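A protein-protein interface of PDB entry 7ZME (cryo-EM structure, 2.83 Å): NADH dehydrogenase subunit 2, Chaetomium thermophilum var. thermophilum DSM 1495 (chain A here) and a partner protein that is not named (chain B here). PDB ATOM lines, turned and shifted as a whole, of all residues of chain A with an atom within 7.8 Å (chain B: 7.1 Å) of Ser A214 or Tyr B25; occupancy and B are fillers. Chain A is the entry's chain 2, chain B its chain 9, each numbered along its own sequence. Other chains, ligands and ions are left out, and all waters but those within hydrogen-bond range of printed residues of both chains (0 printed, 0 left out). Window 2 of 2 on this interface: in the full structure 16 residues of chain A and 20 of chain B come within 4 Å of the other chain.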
ATOM      1  N   ASP A 207      17.259 -12.410 -26.365  1.00  0.00           N
ATOM      2  CA  ASP A 207      17.872 -13.718 -26.537  1.00  0.00           C
ATOM      3  C   ASP A 207      18.859 -13.699 -27.700  1.00  0.00           C
ATOM      4  O   ASP A 207      19.964 -14.244 -27.598  1.00  0.00           O
ATOM      5  CB  ASP A 207      16.767 -14.750 -26.754  1.00  0.00           C
ATOM      6  CG  ASP A 207      17.265 -16.176 -26.728  1.00  0.00           C
ATOM      7  OD1 ASP A 207      18.481 -16.395 -26.570  1.00  0.00           O
ATOM      8  OD2 ASP A 207      16.420 -17.085 -26.861  1.00  0.00           O
ATOM      9  N   GLY A 208      18.480 -13.061 -28.809  1.00  0.00           N
ATOM     10  CA  GLY A 208      19.418 -12.842 -29.895  1.00  0.00           C
ATOM     11  C   GLY A 208      20.539 -11.882 -29.562  1.00  0.00           C
ATOM     12  O   GLY A 208      21.667 -12.064 -30.026  1.00  0.00           O
ATOM     13  N   LEU A 209      20.255 -10.844 -28.772  1.00  0.00           N
ATOM     14  CA  LEU A 209      21.307  -9.928 -28.342  1.00  0.00           C
ATOM     15  C   LEU A 209      22.327 -10.626 -27.454  1.00  0.00           C
ATOM     16  O   LEU A 209      23.523 -10.323 -27.516  1.00  0.00           O
ATOM     17  CB  LEU A 209      20.700  -8.732 -27.611  1.00  0.00           C
ATOM     18  CG  LEU A 209      19.933  -7.710 -28.448  1.00  0.00           C
ATOM     19  CD1 LEU A 209      19.181  -6.737 -27.560  1.00  0.00           C
ATOM     20  CD2 LEU A 209      20.904  -6.966 -29.337  1.00  0.00           C
ATOM     21  N   TYR A 210      21.869 -11.555 -26.611  1.00  0.00           N
ATOM     22  CA  TYR A 210      22.782 -12.284 -25.738  1.00  0.00           C
ATOM     23  C   TYR A 210      23.749 -13.142 -26.539  1.00  0.00           C
ATOM     24  O   TYR A 210      24.934 -13.234 -26.202  1.00  0.00           O
ATOM     25  CB  TYR A 210      21.992 -13.147 -24.759  1.00  0.00           C
ATOM     26  CG  TYR A 210      21.183 -12.360 -23.762  1.00  0.00           C
ATOM     27  CD1 TYR A 210      21.518 -11.053 -23.444  1.00  0.00           C
ATOM     28  CD2 TYR A 210      20.080 -12.922 -23.137  1.00  0.00           C
ATOM     29  CE1 TYR A 210      20.779 -10.325 -22.533  1.00  0.00           C
ATOM     30  CE2 TYR A 210      19.336 -12.204 -22.222  1.00  0.00           C
ATOM     31  CZ  TYR A 210      19.692 -10.906 -21.925  1.00  0.00           C
ATOM     32  OH  TYR A 210      18.959 -10.182 -21.018  1.00  0.00           O
ATOM     33  N   ILE A 211      23.261 -13.791 -27.597  1.00  0.00           N
ATOM     34  CA  ILE A 211      24.119 -14.658 -28.396  1.00  0.00           C
ATOM     35  C   ILE A 211      25.163 -13.840 -29.145  1.00  0.00           C
ATOM     36  O   ILE A 211      26.329 -14.239 -29.236  1.00  0.00           O
ATOM     37  CB  ILE A 211      23.269 -15.518 -29.347  1.00  0.00           C
ATOM     38  CG1 ILE A 211      22.602 -16.647 -28.570  1.00  0.00           C
ATOM     39  CG2 ILE A 211      24.116 -16.095 -30.462  1.00  0.00           C
ATOM     40  CD1 ILE A 211      21.919 -17.648 -29.439  1.00  0.00           C
ATOM     41  N   LEU A 212      24.773 -12.690 -29.689  1.00  0.00           N
ATOM     42  CA  LEU A 212      25.759 -11.805 -30.366  1.00  0.00           C
ATOM     43  C   LEU A 212      26.842 -11.373 -29.366  1.00  0.00           C
ATOM     44  O   LEU A 212      28.009 -11.361 -29.757  1.00  0.00           O
ATOM     45  CB  LEU A 212      25.036 -10.605 -30.982  1.00  0.00           C
ATOM     46  CG  LEU A 212      24.088 -10.909 -32.140  1.00  0.00           C
ATOM     47  CD1 LEU A 212      23.187  -9.720 -32.420  1.00  0.00           C
ATOM     48  CD2 LEU A 212      24.860 -11.296 -33.389  1.00  0.00           C
ATOM     49  N   ASN A 213      26.466 -11.039 -28.132  1.00  0.00           N
ATOM     50  CA  ASN A 213      27.424 -10.673 -27.057  1.00  0.00           C
ATOM     51  C   ASN A 213      28.299 -11.870 -26.694  1.00  0.00           C
ATOM     52  O   ASN A 213      29.487 -11.665 -26.404  1.00  0.00           O
ATOM     53  CB  ASN A 213      26.698 -10.172 -25.807  1.00  0.00           C
ATOM     54  CG  ASN A 213      27.585 -10.071 -24.585  1.00  0.00           C
ATOM     55  OD1 ASN A 213      27.314 -10.697 -23.566  1.00  0.00           O
ATOM     56  ND2 ASN A 213      28.653  -9.297 -24.678  1.00  0.00           N
ATOM     57  N   SER A 214      27.751 -13.078 -26.734  1.00  0.00           N
ATOM     58  CA  SER A 214      28.513 -14.256 -26.271  1.00  0.00           C
ATOM     59  C   SER A 214      29.520 -14.656 -27.350  1.00  0.00           C
ATOM     60  O   SER A 214      30.690 -14.846 -27.004  1.00  0.00           O
ATOM     61  CB  SER A 214      27.587 -15.382 -25.961  1.00  0.00           C
ATOM     62  OG  SER A 214      28.301 -16.514 -25.494  1.00  0.00           O
ATOM     63  N   ILE A 215      29.093 -14.715 -28.616  1.00  0.00           N
ATOM     64  CA  ILE A 215      30.043 -15.034 -29.678  1.00  0.00           C
ATOM     65  C   ILE A 215      31.177 -14.023 -29.692  1.00  0.00           C
ATOM     66  O   ILE A 215      32.352 -14.382 -29.832  1.00  0.00           O
ATOM     67  CB  ILE A 215      29.329 -15.087 -31.042  1.00  0.00           C
ATOM     68  CG1 ILE A 215      28.230 -16.144 -31.049  1.00  0.00           C
ATOM     69  CG2 ILE A 215      30.310 -15.373 -32.150  1.00  0.00           C
ATOM     70  CD1 ILE A 215      27.330 -16.063 -32.257  1.00  0.00           C
ATOM     71  N   SER A 216      30.788 -12.748 -29.645  1.00  0.00           N
ATOM     72  CA  SER A 216      31.752 -11.622 -29.697  1.00  0.00           C
ATOM     73  C   SER A 216      32.849 -11.776 -28.651  1.00  0.00           C
ATOM     74  O   SER A 216      33.961 -11.291 -28.903  1.00  0.00           O
ATOM     75  CB  SER A 216      31.035 -10.328 -29.526  1.00  0.00           C
ATOM     76  OG  SER A 216      30.715 -10.099 -28.166  1.00  0.00           O
ATOM     77  N   ASP A 217      32.538 -12.374 -27.503  1.00  0.00           N
ATOM     78  CA  ASP A 217      33.570 -12.451 -26.447  1.00  0.00           C
ATOM     79  C   ASP A 217      34.523 -13.562 -26.871  1.00  0.00           C
ATOM     80  O   ASP A 217      34.125 -14.735 -26.829  1.00  0.00           O
ATOM     81  CB  ASP A 217      32.938 -12.728 -25.083  1.00  0.00           C
ATOM     82  CG  ASP A 217      33.932 -12.703 -23.935  1.00  0.00           C
ATOM     83  OD1 ASP A 217      34.993 -12.067 -24.094  1.00  0.00           O
ATOM     84  OD2 ASP A 217      33.639 -13.323 -22.894  1.00  0.00           O
ATOM     85  N   VAL A 218      35.746 -13.200 -27.244  1.00  0.00           N
ATOM     86  CA  VAL A 218      36.714 -14.208 -27.763  1.00  0.00           C
ATOM     87  C   VAL A 218      37.795 -14.380 -26.698  1.00  0.00           C
ATOM     88  O   VAL A 218      37.925 -15.501 -26.169  1.00  0.00           O
ATOM     89  CB  VAL A 218      37.312 -13.784 -29.116  1.00  0.00           C
ATOM     90  CG1 VAL A 218      38.261 -14.839 -29.664  1.00  0.00           C
ATOM     91  CG2 VAL A 218      36.228 -13.471 -30.137  1.00  0.00           C
ATOM     92  N   LEU A 240      26.826  -2.486 -28.061  1.00  0.00           N
ATOM     93  CA  LEU A 240      26.076  -3.174 -27.016  1.00  0.00           C
ATOM     94  C   LEU A 240      26.287  -2.522 -25.656  1.00  0.00           C
ATOM     95  O   LEU A 240      25.321  -2.192 -24.962  1.00  0.00           O
ATOM     96  CB  LEU A 240      26.465  -4.650 -26.973  1.00  0.00           C
ATOM     97  CG  LEU A 240      26.010  -5.394 -25.718  1.00  0.00           C
ATOM     98  CD1 LEU A 240      24.522  -5.712 -25.774  1.00  0.00           C
ATOM     99  CD2 LEU A 240      26.816  -6.655 -25.543  1.00  0.00           C
ATOM    100  N   TYR A 297      23.541 -12.073 -18.320  1.00  0.00           N
ATOM    101  CA  TYR A 297      23.806 -12.563 -19.693  1.00  0.00           C
ATOM    102  C   TYR A 297      24.887 -11.718 -20.382  1.00  0.00           C
ATOM    103  O   TYR A 297      25.689 -12.292 -21.126  1.00  0.00           O
ATOM    104  CB  TYR A 297      22.502 -12.845 -20.439  1.00  0.00           C
ATOM    105  CG  TYR A 297      21.729 -14.028 -19.923  1.00  0.00           C
ATOM    106  CD1 TYR A 297      22.105 -15.320 -20.243  1.00  0.00           C
ATOM    107  CD2 TYR A 297      20.618 -13.858 -19.117  1.00  0.00           C
ATOM    108  CE1 TYR A 297      21.403 -16.415 -19.771  1.00  0.00           C
ATOM    109  CE2 TYR A 297      19.906 -14.941 -18.636  1.00  0.00           C
ATOM    110  CZ  TYR A 297      20.298 -16.224 -18.964  1.00  0.00           C
ATOM    111  OH  TYR A 297      19.591 -17.289 -18.488  1.00  0.00           O
ATOM    112  N   THR A 298      24.928 -10.412 -20.131  1.00  0.00           N
ATOM    113  CA  THR A 298      25.871  -9.527 -20.859  1.00  0.00           C
ATOM    114  C   THR A 298      27.256  -9.475 -20.210  1.00  0.00           C
ATOM    115  O   THR A 298      28.110  -8.757 -20.753  1.00  0.00           O
ATOM    116  CB  THR A 298      25.288  -8.122 -21.041  1.00  0.00           C
ATOM    117  OG1 THR A 298      25.056  -7.582 -19.742  1.00  0.00           O
ATOM    118  CG2 THR A 298      24.011  -8.118 -21.853  1.00  0.00           C
ATOM    119  N   ASN A 299      27.481 -10.173 -19.096  1.00  0.00           N
ATOM    120  CA  ASN A 299      28.850 -10.198 -18.522  1.00  0.00           C
ATOM    121  C   ASN A 299      29.777 -10.956 -19.455  1.00  0.00           C
ATOM    122  O   ASN A 299      29.383 -12.040 -19.916  1.00  0.00           O
ATOM    123  CB  ASN A 299      28.932 -10.865 -17.154  1.00  0.00           C
ATOM    124  CG  ASN A 299      29.280  -9.906 -16.037  1.00  0.00           C
ATOM    125  OD1 ASN A 299      28.954  -8.725 -16.101  1.00  0.00           O
ATOM    126  ND2 ASN A 299      29.935 -10.410 -15.006  1.00  0.00           N
ATOM    127  N   SER A 300      30.985 -10.430 -19.668  1.00  0.00           N
ATOM    128  CA  SER A 300      31.984 -11.154 -20.492  1.00  0.00           C
ATOM    129  C   SER A 300      32.851 -11.998 -19.556  1.00  0.00           C
ATOM    130  O   SER A 300      33.493 -11.413 -18.665  1.00  0.00           O
ATOM    131  CB  SER A 300      32.820 -10.193 -21.290  1.00  0.00           C
ATOM    132  OG  SER A 300      32.015  -9.456 -22.197  1.00  0.00           O
ATOM    133  N   ASN A 301      32.860 -13.320 -19.752  1.00  0.00           N
ATOM    134  CA  ASN A 301      33.623 -14.222 -18.848  1.00  0.00           C
ATOM    135  C   ASN A 301      35.108 -14.137 -19.205  1.00  0.00           C
ATOM    136  O   ASN A 301      35.931 -14.652 -18.425  1.00  0.00           O
ATOM    137  CB  ASN A 301      33.087 -15.655 -18.889  1.00  0.00           C
ATOM    138  CG  ASN A 301      31.712 -15.784 -18.266  1.00  0.00           C
ATOM    139  OD1 ASN A 301      31.023 -14.789 -18.053  1.00  0.00           O
ATOM    140  ND2 ASN A 301      31.305 -17.007 -17.971  1.00  0.00           N
ATOM    141  N   LEU A 306      36.069  -5.105 -24.789  1.00  0.00           N
ATOM    142  CA  LEU A 306      34.667  -4.872 -24.454  1.00  0.00           C
ATOM    143  C   LEU A 306      34.476  -4.723 -22.951  1.00  0.00           C
ATOM    144  O   LEU A 306      33.654  -3.916 -22.498  1.00  0.00           O
ATOM    145  CB  LEU A 306      33.801  -6.011 -24.992  1.00  0.00           C
ATOM    146  CG  LEU A 306      33.836  -6.257 -26.501  1.00  0.00           C
ATOM    147  CD1 LEU A 306      32.932  -7.423 -26.861  1.00  0.00           C
ATOM    148  CD2 LEU A 306      33.431  -5.004 -27.264  1.00  0.00           C
ATOM    149  N   GLN B  19      19.691 -17.028 -39.376  1.00  0.00           N
ATOM    150  CA  GLN B  19      19.305 -18.428 -39.073  1.00  0.00           C
ATOM    151  C   GLN B  19      20.563 -19.287 -39.093  1.00  0.00           C
ATOM    152  O   GLN B  19      20.655 -20.194 -38.267  1.00  0.00           O
ATOM    153  CB  GLN B  19      18.193 -18.900 -40.010  1.00  0.00           C
ATOM    154  CG  GLN B  19      16.855 -18.244 -39.737  1.00  0.00           C
ATOM    155  CD  GLN B  19      15.964 -19.080 -38.853  1.00  0.00           C
ATOM    156  OE1 GLN B  19      15.415 -20.090 -39.278  1.00  0.00           O
ATOM    157  NE2 GLN B  19      15.790 -18.646 -37.615  1.00  0.00           N
ATOM    158  N   GLU B  20      21.494 -18.992 -39.990  1.00  0.00           N
ATOM    159  CA  GLU B  20      22.770 -19.742 -40.022  1.00  0.00           C
ATOM    160  C   GLU B  20      23.588 -19.492 -38.749  1.00  0.00           C
ATOM    161  O   GLU B  20      24.165 -20.445 -38.232  1.00  0.00           O
ATOM    162  CB  GLU B  20      23.527 -19.457 -41.322  1.00  0.00           C
ATOM    163  CG  GLU B  20      24.786 -20.289 -41.471  1.00  0.00           C
ATOM    164  CD  GLU B  20      25.695 -19.858 -42.605  1.00  0.00           C
ATOM    165  OE1 GLU B  20      26.750 -20.492 -42.790  1.00  0.00           O
ATOM    166  OE2 GLU B  20      25.342 -18.887 -43.299  1.00  0.00           O
ATOM    167  N   LEU B  21      23.650 -18.259 -38.277  1.00  0.00           N
ATOM    168  CA  LEU B  21      24.410 -17.929 -37.053  1.00  0.00           C
ATOM    169  C   LEU B  21      23.817 -18.616 -35.819  1.00  0.00           C
ATOM    170  O   LEU B  21      24.599 -19.162 -35.023  1.00  0.00           O
ATOM    171  CB  LEU B  21      24.400 -16.409 -36.906  1.00  0.00           C
ATOM    172  CG  LEU B  21      25.139 -15.839 -35.704  1.00  0.00           C
ATOM    173  CD1 LEU B  21      26.587 -16.295 -35.707  1.00  0.00           C
ATOM    174  CD2 LEU B  21      25.045 -14.324 -35.702  1.00  0.00           C
ATOM    175  N   LEU B  22      22.497 -18.597 -35.661  1.00  0.00           N
ATOM    176  CA  LEU B  22      21.829 -19.260 -34.519  1.00  0.00           C
ATOM    177  C   LEU B  22      22.026 -20.759 -34.634  1.00  0.00           C
ATOM    178  O   LEU B  22      22.185 -21.419 -33.601  1.00  0.00           O
ATOM    179  CB  LEU B  22      20.339 -18.933 -34.538  1.00  0.00           C
ATOM    180  CG  LEU B  22      19.926 -17.523 -34.126  1.00  0.00           C
ATOM    181  CD1 LEU B  22      18.412 -17.406 -34.133  1.00  0.00           C
ATOM    182  CD2 LEU B  22      20.466 -17.177 -32.753  1.00  0.00           C
ATOM    183  N   ALA B  23      21.941 -21.284 -35.853  1.00  0.00           N
ATOM    184  CA  ALA B  23      22.108 -22.733 -36.066  1.00  0.00           C
ATOM    185  C   ALA B  23      23.519 -23.100 -35.660  1.00  0.00           C
ATOM    186  O   ALA B  23      23.673 -24.083 -34.945  1.00  0.00           O
ATOM    187  CB  ALA B  23      21.881 -23.034 -37.508  1.00  0.00           C
ATOM    188  N   CYS B  24      24.495 -22.292 -36.079  1.00  0.00           N
ATOM    189  CA  CYS B  24      25.916 -22.516 -35.730  1.00  0.00           C
ATOM    190  C   CYS B  24      26.056 -22.484 -34.206  1.00  0.00           C
ATOM    191  O   CYS B  24      26.745 -23.340 -33.677  1.00  0.00           O
ATOM    192  CB  CYS B  24      26.771 -21.443 -36.394  1.00  0.00           C
ATOM    193  SG  CYS B  24      28.552 -21.741 -36.412  1.00  0.00           S
ATOM    194  N   TYR B  25      25.445 -21.513 -33.534  1.00  0.00           N
ATOM    195  CA  TYR B  25      25.655 -21.409 -32.062  1.00  0.00           C
ATOM    196  C   TYR B  25      25.132 -22.659 -31.354  1.00  0.00           C
ATOM    197  O   TYR B  25      25.899 -23.292 -30.628  1.00  0.00           O
ATOM    198  CB  TYR B  25      25.018 -20.137 -31.494  1.00  0.00           C
ATOM    199  CG  TYR B  25      25.426 -19.810 -30.080  1.00  0.00           C
ATOM    200  CD1 TYR B  25      26.577 -19.087 -29.821  1.00  0.00           C
ATOM    201  CD2 TYR B  25      24.666 -20.225 -29.000  1.00  0.00           C
ATOM    202  CE1 TYR B  25      26.961 -18.778 -28.528  1.00  0.00           C
ATOM    203  CE2 TYR B  25      25.040 -19.932 -27.701  1.00  0.00           C
ATOM    204  CZ  TYR B  25      26.190 -19.204 -27.463  1.00  0.00           C
ATOM    205  OH  TYR B  25      26.564 -18.910 -26.185  1.00  0.00           O
ATOM    206  N   VAL B  26      23.870 -23.006 -31.589  1.00  0.00           N
ATOM    207  CA  VAL B  26      23.220 -24.183 -30.946  1.00  0.00           C
ATOM    208  C   VAL B  26      23.959 -25.469 -31.333  1.00  0.00           C
ATOM    209  O   VAL B  26      24.030 -26.369 -30.484  1.00  0.00           O
ATOM    210  CB  VAL B  26      21.727 -24.215 -31.323  1.00  0.00           C
ATOM    211  CG1 VAL B  26      21.007 -25.447 -30.812  1.00  0.00           C
ATOM    212  CG2 VAL B  26      21.011 -22.951 -30.884  1.00  0.00           C
ATOM    213  N   THR B  27      24.516 -25.555 -32.539  1.00  0.00           N
ATOM    214  CA  THR B  27      25.126 -26.828 -32.990  1.00  0.00           C
ATOM    215  C   THR B  27      26.627 -26.898 -32.705  1.00  0.00           C
ATOM    216  O   THR B  27      27.218 -27.936 -33.035  1.00  0.00           O
ATOM    217  CB  THR B  27      24.824 -27.122 -34.463  1.00  0.00           C
ATOM    218  OG1 THR B  27      25.378 -26.090 -35.280  1.00  0.00           O
ATOM    219  CG2 THR B  27      23.345 -27.299 -34.736  1.00  0.00           C
ATOM    220  N   ASN B  28      27.220 -25.859 -32.127  1.00  0.00           N
ATOM    221  CA  ASN B  28      28.630 -25.920 -31.760  1.00  0.00           C
ATOM    222  C   ASN B  28      28.888 -25.584 -30.303  1.00  0.00           C
ATOM    223  O   ASN B  28      29.706 -26.245 -29.660  1.00  0.00           O
ATOM    224  CB  ASN B  28      29.455 -24.980 -32.648  1.00  0.00           C
ATOM    225  CG  ASN B  28      29.284 -25.274 -34.120  1.00  0.00           C
ATOM    226  OD1 ASN B  28      29.091 -24.368 -34.925  1.00  0.00           O
ATOM    227  ND2 ASN B  28      29.356 -26.547 -34.482  1.00  0.00           N
ATOM    228  N   SER B  29      28.215 -24.580 -29.760  1.00  0.00           N
ATOM    229  CA  SER B  29      28.437 -24.187 -28.378  1.00  0.00           C
ATOM    230  C   SER B  29      27.731 -25.141 -27.423  1.00  0.00           C
ATOM    231  O   SER B  29      26.685 -25.715 -27.737  1.00  0.00           O
ATOM    232  CB  SER B  29      27.953 -22.758 -28.142  1.00  0.00           C
ATOM    233  OG  SER B  29      27.854 -22.471 -26.760  1.00  0.00           O
ATOM    234  N   SER B  30      28.323 -25.303 -26.248  1.00  0.00           N
ATOM    235  CA  SER B  30      27.777 -26.129 -25.182  1.00  0.00           C
ATOM    236  C   SER B  30      28.582 -25.828 -23.930  1.00  0.00           C
ATOM    237  O   SER B  30      29.624 -25.172 -23.987  1.00  0.00           O
ATOM    238  CB  SER B  30      27.828 -27.619 -25.528  1.00  0.00           C
ATOM    239  OG  SER B  30      29.153 -28.031 -25.818  1.00  0.00           O
ATOM    240  N   PRO B  34      33.108 -24.686 -24.022  1.00  0.00           N
ATOM    241  CA  PRO B  34      32.773 -23.260 -24.155  1.00  0.00           C
ATOM    242  C   PRO B  34      33.307 -22.630 -25.428  1.00  0.00           C
ATOM    243  O   PRO B  34      32.641 -21.760 -26.005  1.00  0.00           O
ATOM    244  CB  PRO B  34      33.408 -22.630 -22.906  1.00  0.00           C
ATOM    245  CG  PRO B  34      33.675 -23.771 -21.974  1.00  0.00           C
ATOM    246  CD  PRO B  34      33.939 -24.956 -22.839  1.00  0.00           C
ATOM    247  N   GLY B  36      33.577 -23.707 -28.408  1.00  0.00           N
ATOM    248  CA  GLY B  36      33.021 -24.128 -29.681  1.00  0.00           C
ATOM    249  C   GLY B  36      32.341 -23.010 -30.435  1.00  0.00           C
ATOM    250  O   GLY B  36      32.155 -23.118 -31.650  1.00  0.00           O
ATOM    251  N   LYS B  37      31.978 -21.937 -29.742  1.00  0.00           N
ATOM    252  CA  LYS B  37      31.302 -20.795 -30.338  1.00  0.00           C
ATOM    253  C   LYS B  37      32.243 -19.879 -31.104  1.00  0.00           C
ATOM    254  O   LYS B  37      31.786 -18.878 -31.662  1.00  0.00           O
ATOM    255  CB  LYS B  37      30.568 -20.010 -29.250  1.00  0.00           C
ATOM    256  CG  LYS B  37      31.485 -19.326 -28.264  1.00  0.00           C
ATOM    257  CD  LYS B  37      30.695 -18.596 -27.210  1.00  0.00           C
ATOM    258  CE  LYS B  37      31.615 -17.949 -26.203  1.00  0.00           C
ATOM    259  NZ  LYS B  37      32.416 -16.854 -26.810  1.00  0.00           N
ATOM    260  N   ASN B  38      33.541 -20.184 -31.131  1.00  0.00           N
ATOM    261  CA  ASN B  38      34.458 -19.469 -32.010  1.00  0.00           C
ATOM    262  C   ASN B  38      34.241 -19.841 -33.467  1.00  0.00           C
ATOM    263  O   ASN B  38      34.657 -19.094 -34.356  1.00  0.00           O
ATOM    264  CB  ASN B  38      35.898 -19.755 -31.603  1.00  0.00           C
ATOM    265  CG  ASN B  38      36.177 -19.379 -30.166  1.00  0.00           C
ATOM    266  OD1 ASN B  38      35.262 -19.064 -29.408  1.00  0.00           O
ATOM    267  ND2 ASN B  38      37.447 -19.410 -29.781  1.00  0.00           N
ATOM    268  N   CYS B  40      31.498 -19.581 -34.719  1.00  0.00           N
ATOM    269  CA  CYS B  40      30.468 -18.629 -35.095  1.00  0.00           C
ATOM    270  C   CYS B  40      31.031 -17.267 -35.476  1.00  0.00           C
ATOM    271  O   CYS B  40      30.267 -16.400 -35.907  1.00  0.00           O
ATOM    272  CB  CYS B  40      29.478 -18.465 -33.943  1.00  0.00           C
ATOM    273  SG  CYS B  40      28.661 -19.976 -33.422  1.00  0.00           S
ATOM    274  N   ILE B  41      32.337 -17.054 -35.316  1.00  0.00           N
ATOM    275  CA  ILE B  41      32.914 -15.739 -35.602  1.00  0.00           C
ATOM    276  C   ILE B  41      32.750 -15.341 -37.064  1.00  0.00           C
ATOM    277  O   ILE B  41      32.299 -14.214 -37.326  1.00  0.00           O
ATOM    278  CB  ILE B  41      34.382 -15.695 -35.140  1.00  0.00           C
ATOM    279  CG1 ILE B  41      34.488 -15.979 -33.645  1.00  0.00           C
ATOM    280  CG2 ILE B  41      34.994 -14.345 -35.452  1.00  0.00           C
ATOM    281  CD1 ILE B  41      33.768 -14.988 -32.790  1.00  0.00           C
ATOM    282  N   VAL B  43      30.568 -16.563 -39.161  1.00  0.00           N
ATOM    283  CA  VAL B  43      29.129 -16.563 -39.383  1.00  0.00           C
ATOM    284  C   VAL B  43      28.501 -15.290 -38.833  1.00  0.00           C
ATOM    285  O   VAL B  43      27.550 -14.753 -39.410  1.00  0.00           O
ATOM    286  CB  VAL B  43      28.514 -17.825 -38.754  1.00  0.00           C
ATOM    287  CG1 VAL B  43      27.109 -18.018 -39.224  1.00  0.00           C
ATOM    288  CG2 VAL B  43      29.349 -19.036 -39.101  1.00  0.00           C
ATOM    289  N   MET B  44      29.023 -14.786 -37.712  1.00  0.00           N
ATOM    290  CA  MET B  44      28.479 -13.568 -37.122  1.00  0.00           C
ATOM    291  C   MET B  44      28.923 -12.333 -37.889  1.00  0.00           C
ATOM    292  O   MET B  44      28.202 -11.332 -37.923  1.00  0.00           O
ATOM    293  CB  MET B  44      28.887 -13.468 -35.650  1.00  0.00           C
ATOM    294  CG  MET B  44      28.186 -12.352 -34.878  1.00  0.00           C
ATOM    295  SD  MET B  44      28.888 -12.028 -33.254  1.00  0.00           S
ATOM    296  CE  MET B  44      30.624 -11.916 -33.659  1.00  0.00           C
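Ser A214 touches just these residues of chain B: Tyr B25 (3.0 Å) and Lys B37 (2.7 Å). Of chain A, only Ile A211, Ser A214 and Ile A215 come within 4 Å of Tyr B25. Printed residues of chain A within 4 Å of Met B44: Leu A212 and Ile A215. Of the printed residues of chain B, Leu A212 touches Leu B21 and Met B44. Thr A298 touches none of the printed residues of chain B. The nearest residue of chain B that does not touch Ser A214 is Ser B29 (6.1 Å). The nearest residue of chain A that does not touch Tyr B25 is Tyr A210 (5.9 Å). The nearest printed residue of chain B that does not touch Ile A211 is Met B44 (5.3 Å).
Leu B22 touches Ile A211 (CD2 to CD1, 3.6 Å). CD1 of Ile A211 touches CD2 of Tyr B25, 3.8 Å away. Leu A212 touches Leu B21. Ile A215 touches Leu B21 (CD1 to CD1, 3.5 Å). Ile A215 touches Tyr B25 (CG1 to CD1, 3.6 Å). Ile A215 touches Lys B37 (CG2 to O, 3.8 Å). Ile A215 touches Cys B40. Ile A215 touches Ile B41. CG2 of Ile A215 touches CE of Met B44, at 3.8 Å. Ile B41 touches Val A218 (CD1 to CG2, 3.9 Å).
The side-chain amino group (NZ) of Lys B37 is in hydrogen-bond range of the backbone carbonyl oxygen (O) of Ser A214 (2.7 Å). OG of Ser A214 is in hydrogen-bond range of OH of Tyr B25 (3.0 Å). O of Leu A212 sits close to SD of Met B44, at 3.7 Å. The backbone carbonyl oxygen (O) of Asp A217 lies within hydrogen-bond range of the side-chain amino group (NZ) of Lys B37, at 2.7 Å.
The side-chain carboxylate of Asp A217 is in hydrogen-bond range of the backbone NH of Asn A301 (3.2 Å). The side-chain sulfur of Cys B40 lies within hydrogen-bond range of the side-chain sulfur of Cys B24 (3.5 Å). O of Leu A212 sits close to OG of Ser A216 (3.4 Å). The side-chain sulfur (SG) of Cys B40 sits at hydrogen-bond distance from the backbone NH (N) of Tyr B25. O of Lys B37 lies close to SG of Cys B40 (3.8 Å).
Printed residues of chain A that touch a printed residue of chain B: Ile A211, Leu A212, Ser A214, Ile A215, Asp A217 and Val A218. Hydrophobic or aromatic side chains of chain A within 4 Å of the printed part of chain B: Ile A211, Leu A212, Ile A215 and Val A218. Of the 20 printed residues of chain B, 7 touch a printed residue of chain A. Along chain B the printed residues that touch a printed residue of chain A span positions 21 to 44.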
